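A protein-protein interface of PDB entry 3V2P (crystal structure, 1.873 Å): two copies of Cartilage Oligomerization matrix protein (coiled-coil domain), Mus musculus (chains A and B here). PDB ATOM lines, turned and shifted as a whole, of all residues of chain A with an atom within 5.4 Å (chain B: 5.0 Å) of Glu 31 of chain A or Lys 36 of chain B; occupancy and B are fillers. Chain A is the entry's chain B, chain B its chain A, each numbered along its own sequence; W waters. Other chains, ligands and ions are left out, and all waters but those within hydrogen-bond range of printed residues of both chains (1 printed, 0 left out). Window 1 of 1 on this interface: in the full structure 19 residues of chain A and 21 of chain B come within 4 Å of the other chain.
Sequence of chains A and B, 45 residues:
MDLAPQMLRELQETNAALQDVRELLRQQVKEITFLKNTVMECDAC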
ATOM      1  N   GLN A  27      -3.535  25.486 -16.309  1.00  0.00           N
ATOM      2  CA  GLN A  27      -3.507  26.638 -17.198  1.00  0.00           C
ATOM      3  C   GLN A  27      -2.843  26.269 -18.522  1.00  0.00           C
ATOM      4  O   GLN A  27      -3.245  26.747 -19.580  1.00  0.00           O
ATOM      5  CB  GLN A  27      -2.786  27.827 -16.545  1.00  0.00           C
ATOM      6  CG  GLN A  27      -1.327  27.605 -16.196  1.00  0.00           C
ATOM      7  CD  GLN A  27      -0.678  28.835 -15.571  1.00  0.00           C
ATOM      8  OE1 GLN A  27      -0.442  29.843 -16.241  1.00  0.00           O
ATOM      9  NE2 GLN A  27      -0.397  28.758 -14.275  1.00  0.00           N
ATOM     10  N   GLN A  28      -1.847  25.391 -18.471  1.00  0.00           N
ATOM     11  CA  GLN A  28      -1.154  25.005 -19.689  1.00  0.00           C
ATOM     12  C   GLN A  28      -2.064  24.228 -20.636  1.00  0.00           C
ATOM     13  O   GLN A  28      -2.012  24.421 -21.852  1.00  0.00           O
ATOM     14  CB  GLN A  28       0.098  24.191 -19.352  1.00  0.00           C
ATOM     15  CG  GLN A  28       0.957  23.875 -20.571  1.00  0.00           C
ATOM     16  CD  GLN A  28       2.244  23.176 -20.197  1.00  0.00           C
ATOM     17  OE1 GLN A  28       3.290  23.806 -20.038  1.00  0.00           O
ATOM     18  NE2 GLN A  28       2.170  21.870 -20.032  1.00  0.00           N
ATOM     19  N   VAL A  29      -2.905  23.356 -20.085  1.00  0.00           N
ATOM     20  CA  VAL A  29      -3.826  22.589 -20.915  1.00  0.00           C
ATOM     21  C   VAL A  29      -4.803  23.535 -21.603  1.00  0.00           C
ATOM     22  O   VAL A  29      -5.208  23.302 -22.740  1.00  0.00           O
ATOM     23  CB  VAL A  29      -4.642  21.577 -20.074  1.00  0.00           C
ATOM     24  CG1 VAL A  29      -5.686  20.894 -20.950  1.00  0.00           C
ATOM     25  CG2 VAL A  29      -3.709  20.553 -19.458  1.00  0.00           C
ATOM     26  N   LYS A  30      -5.183  24.607 -20.911  1.00  0.00           N
ATOM     27  CA  LYS A  30      -6.120  25.566 -21.492  1.00  0.00           C
ATOM     28  C   LYS A  30      -5.499  26.309 -22.675  1.00  0.00           C
ATOM     29  O   LYS A  30      -6.171  26.595 -23.669  1.00  0.00           O
ATOM     30  CB  LYS A  30      -6.574  26.571 -20.431  1.00  0.00           C
ATOM     31  CG  LYS A  30      -7.661  27.508 -20.925  1.00  0.00           C
ATOM     32  CD  LYS A  30      -8.290  28.306 -19.800  1.00  0.00           C
ATOM     33  CE  LYS A  30      -9.480  29.107 -20.322  1.00  0.00           C
ATOM     34  NZ  LYS A  30     -10.183  29.853 -19.240  1.00  0.00           N
ATOM     35  N   GLU A  31      -4.216  26.626 -22.556  1.00  0.00           N
ATOM     36  CA  GLU A  31      -3.491  27.322 -23.614  1.00  0.00           C
ATOM     37  C   GLU A  31      -3.340  26.423 -24.833  1.00  0.00           C
ATOM     38  O   GLU A  31      -3.536  26.861 -25.962  1.00  0.00           O
ATOM     39  CB  GLU A  31      -2.107  27.740 -23.116  1.00  0.00           C
ATOM     40  CG  GLU A  31      -2.148  28.761 -21.998  1.00  0.00           C
ATOM     41  CD  GLU A  31      -2.679  30.101 -22.467  1.00  0.00           C
ATOM     42  OE1 GLU A  31      -1.937  30.829 -23.152  1.00  0.00           O
ATOM     43  OE2 GLU A  31      -3.842  30.421 -22.161  1.00  0.00           O
ATOM     44  N   ILE A  32      -2.979  25.166 -24.598  1.00  0.00           N
ATOM     45  CA  ILE A  32      -2.807  24.206 -25.681  1.00  0.00           C
ATOM     46  C   ILE A  32      -4.136  23.934 -26.376  1.00  0.00           C
ATOM     47  O   ILE A  32      -4.187  23.776 -27.601  1.00  0.00           O
ATOM     48  CB  ILE A  32      -2.234  22.870 -25.158  1.00  0.00           C
ATOM     49  CG1 ILE A  32      -0.815  23.099 -24.627  1.00  0.00           C
ATOM     50  CG2 ILE A  32      -2.246  21.816 -26.278  1.00  0.00           C
ATOM     51  CD1 ILE A  32      -0.194  21.884 -23.957  1.00  0.00           C
ATOM     52  N   THR A  33      -5.207  23.873 -25.588  1.00  0.00           N
ATOM     53  CA  THR A  33      -6.532  23.629 -26.137  1.00  0.00           C
ATOM     54  C   THR A  33      -6.925  24.782 -27.053  1.00  0.00           C
ATOM     55  O   THR A  33      -7.524  24.571 -28.102  1.00  0.00           O
ATOM     56  CB  THR A  33      -7.584  23.486 -25.019  1.00  0.00           C
ATOM     57  OG1 THR A  33      -7.256  22.346 -24.205  1.00  0.00           O
ATOM     58  CG2 THR A  33      -8.981  23.306 -25.623  1.00  0.00           C
ATOM     59  N   PHE A  34      -6.575  25.998 -26.653  1.00  0.00           N
ATOM     60  CA  PHE A  34      -6.879  27.180 -27.452  1.00  0.00           C
ATOM     61  C   PHE A  34      -6.023  27.161 -28.720  1.00  0.00           C
ATOM     62  O   PHE A  34      -6.497  27.480 -29.807  1.00  0.00           O
ATOM     63  CB  PHE A  34      -6.587  28.452 -26.655  1.00  0.00           C
ATOM     64  CG  PHE A  34      -7.151  29.693 -27.281  1.00  0.00           C
ATOM     65  CD1 PHE A  34      -8.444  30.109 -26.983  1.00  0.00           C
ATOM     66  CD2 PHE A  34      -6.405  30.423 -28.200  1.00  0.00           C
ATOM     67  CE1 PHE A  34      -8.989  31.239 -27.593  1.00  0.00           C
ATOM     68  CE2 PHE A  34      -6.942  31.555 -28.816  1.00  0.00           C
ATOM     69  CZ  PHE A  34      -8.236  31.963 -28.511  1.00  0.00           C
ATOM     70  N   LEU A  35      -4.756  26.788 -28.572  1.00  0.00           N
ATOM     71  CA  LEU A  35      -3.841  26.709 -29.708  1.00  0.00           C
ATOM     72  C   LEU A  35      -4.354  25.678 -30.712  1.00  0.00           C
ATOM     73  O   LEU A  35      -4.294  25.898 -31.921  1.00  0.00           O
ATOM     74  CB  LEU A  35      -2.437  26.318 -29.225  1.00  0.00           C
ATOM     75  CG  LEU A  35      -1.351  26.086 -30.281  1.00  0.00           C
ATOM     76  CD1 LEU A  35      -1.260  27.289 -31.213  1.00  0.00           C
ATOM     77  CD2 LEU A  35      -0.017  25.848 -29.582  1.00  0.00           C
ATOM     78  N   LYS A  36      -4.862  24.557 -30.202  1.00  0.00           N
ATOM     79  CA  LYS A  36      -5.405  23.490 -31.044  1.00  0.00           C
ATOM     80  C   LYS A  36      -6.545  24.023 -31.899  1.00  0.00           C
ATOM     81  O   LYS A  36      -6.517  23.926 -33.127  1.00  0.00           O
ATOM     82  CB  LYS A  36      -5.944  22.336 -30.183  1.00  0.00           C
ATOM     83  CG  LYS A  36      -6.609  21.214 -30.988  1.00  0.00           C
ATOM     84  CD  LYS A  36      -7.504  20.317 -30.123  1.00  0.00           C
ATOM     85  CE  LYS A  36      -8.680  21.091 -29.524  1.00  0.00           C
ATOM     86  NZ  LYS A  36      -9.585  20.238 -28.680  1.00  0.00           N
ATOM     87  N   VAL B  29       4.934  27.072 -19.609  1.00  0.00           N
ATOM     88  CA  VAL B  29       3.634  27.701 -19.824  1.00  0.00           C
ATOM     89  C   VAL B  29       3.844  29.048 -20.526  1.00  0.00           C
ATOM     90  O   VAL B  29       3.063  29.436 -21.386  1.00  0.00           O
ATOM     91  CB  VAL B  29       2.869  27.936 -18.498  1.00  0.00           C
ATOM     92  CG1 VAL B  29       1.528  28.585 -18.794  1.00  0.00           C
ATOM     93  CG2 VAL B  29       2.656  26.616 -17.769  1.00  0.00           C
ATOM     94  N   ILE B  32       4.559  28.397 -24.164  1.00  0.00           N
ATOM     95  CA  ILE B  32       3.347  27.952 -24.840  1.00  0.00           C
ATOM     96  C   ILE B  32       2.379  29.109 -25.080  1.00  0.00           C
ATOM     97  O   ILE B  32       1.760  29.199 -26.143  1.00  0.00           O
ATOM     98  CB  ILE B  32       2.643  26.832 -24.033  1.00  0.00           C
ATOM     99  CG1 ILE B  32       3.492  25.559 -24.097  1.00  0.00           C
ATOM    100  CG2 ILE B  32       1.237  26.586 -24.579  1.00  0.00           C
ATOM    101  CD1 ILE B  32       2.938  24.393 -23.307  1.00  0.00           C
ATOM    102  N   THR B  33       2.246  29.993 -24.097  1.00  0.00           N
ATOM    103  CA  THR B  33       1.351  31.135 -24.249  1.00  0.00           C
ATOM    104  C   THR B  33       1.885  32.030 -25.363  1.00  0.00           C
ATOM    105  O   THR B  33       1.121  32.602 -26.148  1.00  0.00           O
ATOM    106  CB  THR B  33       1.255  31.947 -22.946  1.00  0.00           C
ATOM    107  OG1 THR B  33       0.738  31.109 -21.905  1.00  0.00           O
ATOM    108  CG2 THR B  33       0.334  33.143 -23.128  1.00  0.00           C
ATOM    109  N   PHE B  34       3.208  32.140 -25.436  1.00  0.00           N
ATOM    110  CA  PHE B  34       3.835  32.955 -26.462  1.00  0.00           C
ATOM    111  C   PHE B  34       3.560  32.316 -27.818  1.00  0.00           C
ATOM    112  O   PHE B  34       3.226  33.004 -28.779  1.00  0.00           O
ATOM    113  CB  PHE B  34       5.345  33.056 -26.212  1.00  0.00           C
ATOM    114  CG  PHE B  34       6.039  34.034 -27.118  1.00  0.00           C
ATOM    115  CD1 PHE B  34       6.263  33.726 -28.457  1.00  0.00           C
ATOM    116  CD2 PHE B  34       6.428  35.283 -26.644  1.00  0.00           C
ATOM    117  CE1 PHE B  34       6.862  34.652 -29.314  1.00  0.00           C
ATOM    118  CE2 PHE B  34       7.027  36.213 -27.491  1.00  0.00           C
ATOM    119  CZ  PHE B  34       7.242  35.897 -28.828  1.00  0.00           C
ATOM    120  N   LEU B  35       3.697  30.994 -27.882  1.00  0.00           N
ATOM    121  CA  LEU B  35       3.447  30.251 -29.112  1.00  0.00           C
ATOM    122  C   LEU B  35       1.996  30.461 -29.541  1.00  0.00           C
ATOM    123  O   LEU B  35       1.710  30.668 -30.721  1.00  0.00           O
ATOM    124  CB  LEU B  35       3.721  28.758 -28.885  1.00  0.00           C
ATOM    125  CG  LEU B  35       3.422  27.771 -30.017  1.00  0.00           C
ATOM    126  CD1 LEU B  35       4.182  28.171 -31.280  1.00  0.00           C
ATOM    127  CD2 LEU B  35       3.814  26.363 -29.579  1.00  0.00           C
ATOM    128  N   LYS B  36       1.083  30.417 -28.576  1.00  0.00           N
ATOM    129  CA  LYS B  36      -0.330  30.607 -28.871  1.00  0.00           C
ATOM    130  C   LYS B  36      -0.590  31.952 -29.536  1.00  0.00           C
ATOM    131  O   LYS B  36      -1.142  32.015 -30.635  1.00  0.00           O
ATOM    132  CB  LYS B  36      -1.174  30.526 -27.595  1.00  0.00           C
ATOM    133  CG  LYS B  36      -2.664  30.733 -27.867  1.00  0.00           C
ATOM    134  CD  LYS B  36      -3.478  30.870 -26.592  1.00  0.00           C
ATOM    135  CE  LYS B  36      -3.212  32.193 -25.901  1.00  0.00           C
ATOM    136  NZ  LYS B  36      -4.088  32.342 -24.715  1.00  0.00           N
ATOM    137  N   ASN B  37      -0.202  33.026 -28.856  1.00  0.00           N
ATOM    138  CA  ASN B  37      -0.408  34.372 -29.371  1.00  0.00           C
ATOM    139  C   ASN B  37       0.224  34.578 -30.747  1.00  0.00           C
ATOM    140  O   ASN B  37      -0.366  35.218 -31.613  1.00  0.00           O
ATOM    141  CB  ASN B  37       0.133  35.401 -28.373  1.00  0.00           C
ATOM    142  CG  ASN B  37      -0.588  35.344 -27.032  1.00  0.00           C
ATOM    143  OD1 ASN B  37      -1.805  35.170 -26.979  1.00  0.00           O
ATOM    144  ND2 ASN B  37       0.158  35.503 -25.948  1.00  0.00           N
ATOM    145  N   THR B  38       1.419  34.032 -30.951  1.00  0.00           N
ATOM    146  CA  THR B  38       2.095  34.161 -32.240  1.00  0.00           C
ATOM    147  C   THR B  38       1.247  33.511 -33.336  1.00  0.00           C
ATOM    148  O   THR B  38       1.078  34.067 -34.423  1.00  0.00           O
ATOM    149  CB  THR B  38       3.484  33.490 -32.210  1.00  0.00           C
ATOM    150  OG1 THR B  38       4.320  34.163 -31.260  1.00  0.00           O
ATOM    151  CG2 THR B  38       4.136  33.547 -33.577  1.00  0.00           C
ATOM    152  N   VAL B  39       0.710  32.329 -33.038  1.00  0.00           N
ATOM    153  CA  VAL B  39      -0.129  31.596 -33.984  1.00  0.00           C
ATOM    154  C   VAL B  39      -1.429  32.353 -34.250  1.00  0.00           C
ATOM    155  O   VAL B  39      -1.939  32.362 -35.375  1.00  0.00           O
ATOM    156  CB  VAL B  39      -0.458  30.184 -33.444  1.00  0.00           C
ATOM    157  CG1 VAL B  39      -1.477  29.488 -34.341  1.00  0.00           C
ATOM    158  CG2 VAL B  39       0.811  29.364 -33.370  1.00  0.00           C
ATOM    159  N   MET B  40      -1.961  32.988 -33.213  1.00  0.00           N
ATOM    160  CA  MET B  40      -3.194  33.754 -33.342  1.00  0.00           C
ATOM    161  C   MET B  40      -3.004  34.918 -34.313  1.00  0.00           C
ATOM    162  O   MET B  40      -3.946  35.335 -34.990  1.00  0.00           O
ATOM    163  CB  MET B  40      -3.630  34.283 -31.973  1.00  0.00           C
ATOM    164  CG  MET B  40      -4.145  33.212 -31.026  1.00  0.00           C
ATOM    165  SD  MET B  40      -4.427  33.834 -29.351  1.00  0.00           S
ATOM    166  CE  MET B  40      -5.721  35.044 -29.656  1.00  0.00           C
HETATM  167  O   HOH W   1      -1.352  31.454 -19.966  1.00  0.00           O
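Printed residues of chain B within 4 Å of Gln 28 of chain A: Val 29 and Ile 32.
Lys 30 of chain A touches none of the printed residues of chain B.
Of chain B, only Ile 32, Thr 33 and Lys 36 come within 4 Å of Glu 31 of chain A.
Of the printed residues of chain A, Lys 36 of chain B touches Glu 31 (3.1 Å) and Phe 34 (3.4 Å).
Of the printed residues of chain A, Met 40 of chain B touches Phe 34 (3.4 Å).
The nearest printed residue of chain A that does not touch Leu 35 of chain B is Glu 31 of chain A (7.4 Å).
Water W1 lies within hydrogen-bond range of OG1 of Thr 33 of chain B and OE1 of Glu 31 of chain A.
The side-chain hydroxyl (OG1) of Thr 33 of chain B sits at hydrogen-bond distance from the backbone carbonyl oxygen (O) of Val 29 of chain B, at 2.9 Å.
The backbone carbonyl oxygen (O) of Thr 33 of chain B sits at hydrogen-bond distance from the side-chain amide nitrogen (ND2) of Asn 37 of chain B (3.1 Å).
The side-chain amide oxygen (OD1) of Asn 37 of chain B sits close to the side-chain sulfur (SD) of Met 40 of chain B.
Phe 34 of chain A touches Lys 36 of chain B, but with the chains exchanged Lys 36 of chain A does not touch Phe 34 of chain B (11.7 Å).
Leu 35 of chain B touches its own counterpart, Leu 35 of chain A.
Of the 10 pairs that touch across the chains among the printed residues, 1 has its exchanged pair printed and touching as well.
Of the 10 printed residues of chain B, 7 touch a printed residue of chain A.
Printed residues of chain B that touch a printed residue of chain A: Val 29, Ile 32, Thr 33, Leu 35, Lys 36, Val 39 and Met 40.
Hydrophobic or aromatic side chains of chain B within 4 Å of the printed part of chain A: Val 29, Ile 32, Leu 35, Val 39 and Met 40.
Of the 10 printed residues of chain A, 5 touch a printed residue of chain B.
Hydrophobic or aromatic side chains of chain A that line the printed part of chain B: Phe 34 and Leu 35.
Among the printed residues, 10 pairs touch across the chains.
Among the printed residues, Asp or Glu carboxylates within 4 Å of a Lys or Arg side-chain nitrogen of the other chain: Glu 31 of chain A with Lys 36 of chain B.
The side-chain hydroxyl of Thr 33 of chain B lies within hydrogen-bond range of the side-chain carboxylate of Glu 31 of chain A (3.0 Å).
The side-chain amino group (NZ) of Lys 36 of chain B lies within salt-bridge range of the side-chain carboxylate (OE1) of Glu 31 of chain A.
Among the printed residues, merely in contact across the chains: Gln 28 of chain A with Ile 32 of chain B, Phe 34 of chain A with Lys 36 of chain B, Phe 34 of chain A with Met 40 of chain B, Gln 27 of chain A with Val 29 of chain B, Leu 35 of chain A with Val 39 of chain B, Gln 28 of chain A with Val 29 of chain B, Glu 31 of chain A with Ile 32 of chain B and Leu 35 of chain A with Leu 35 of chain B.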
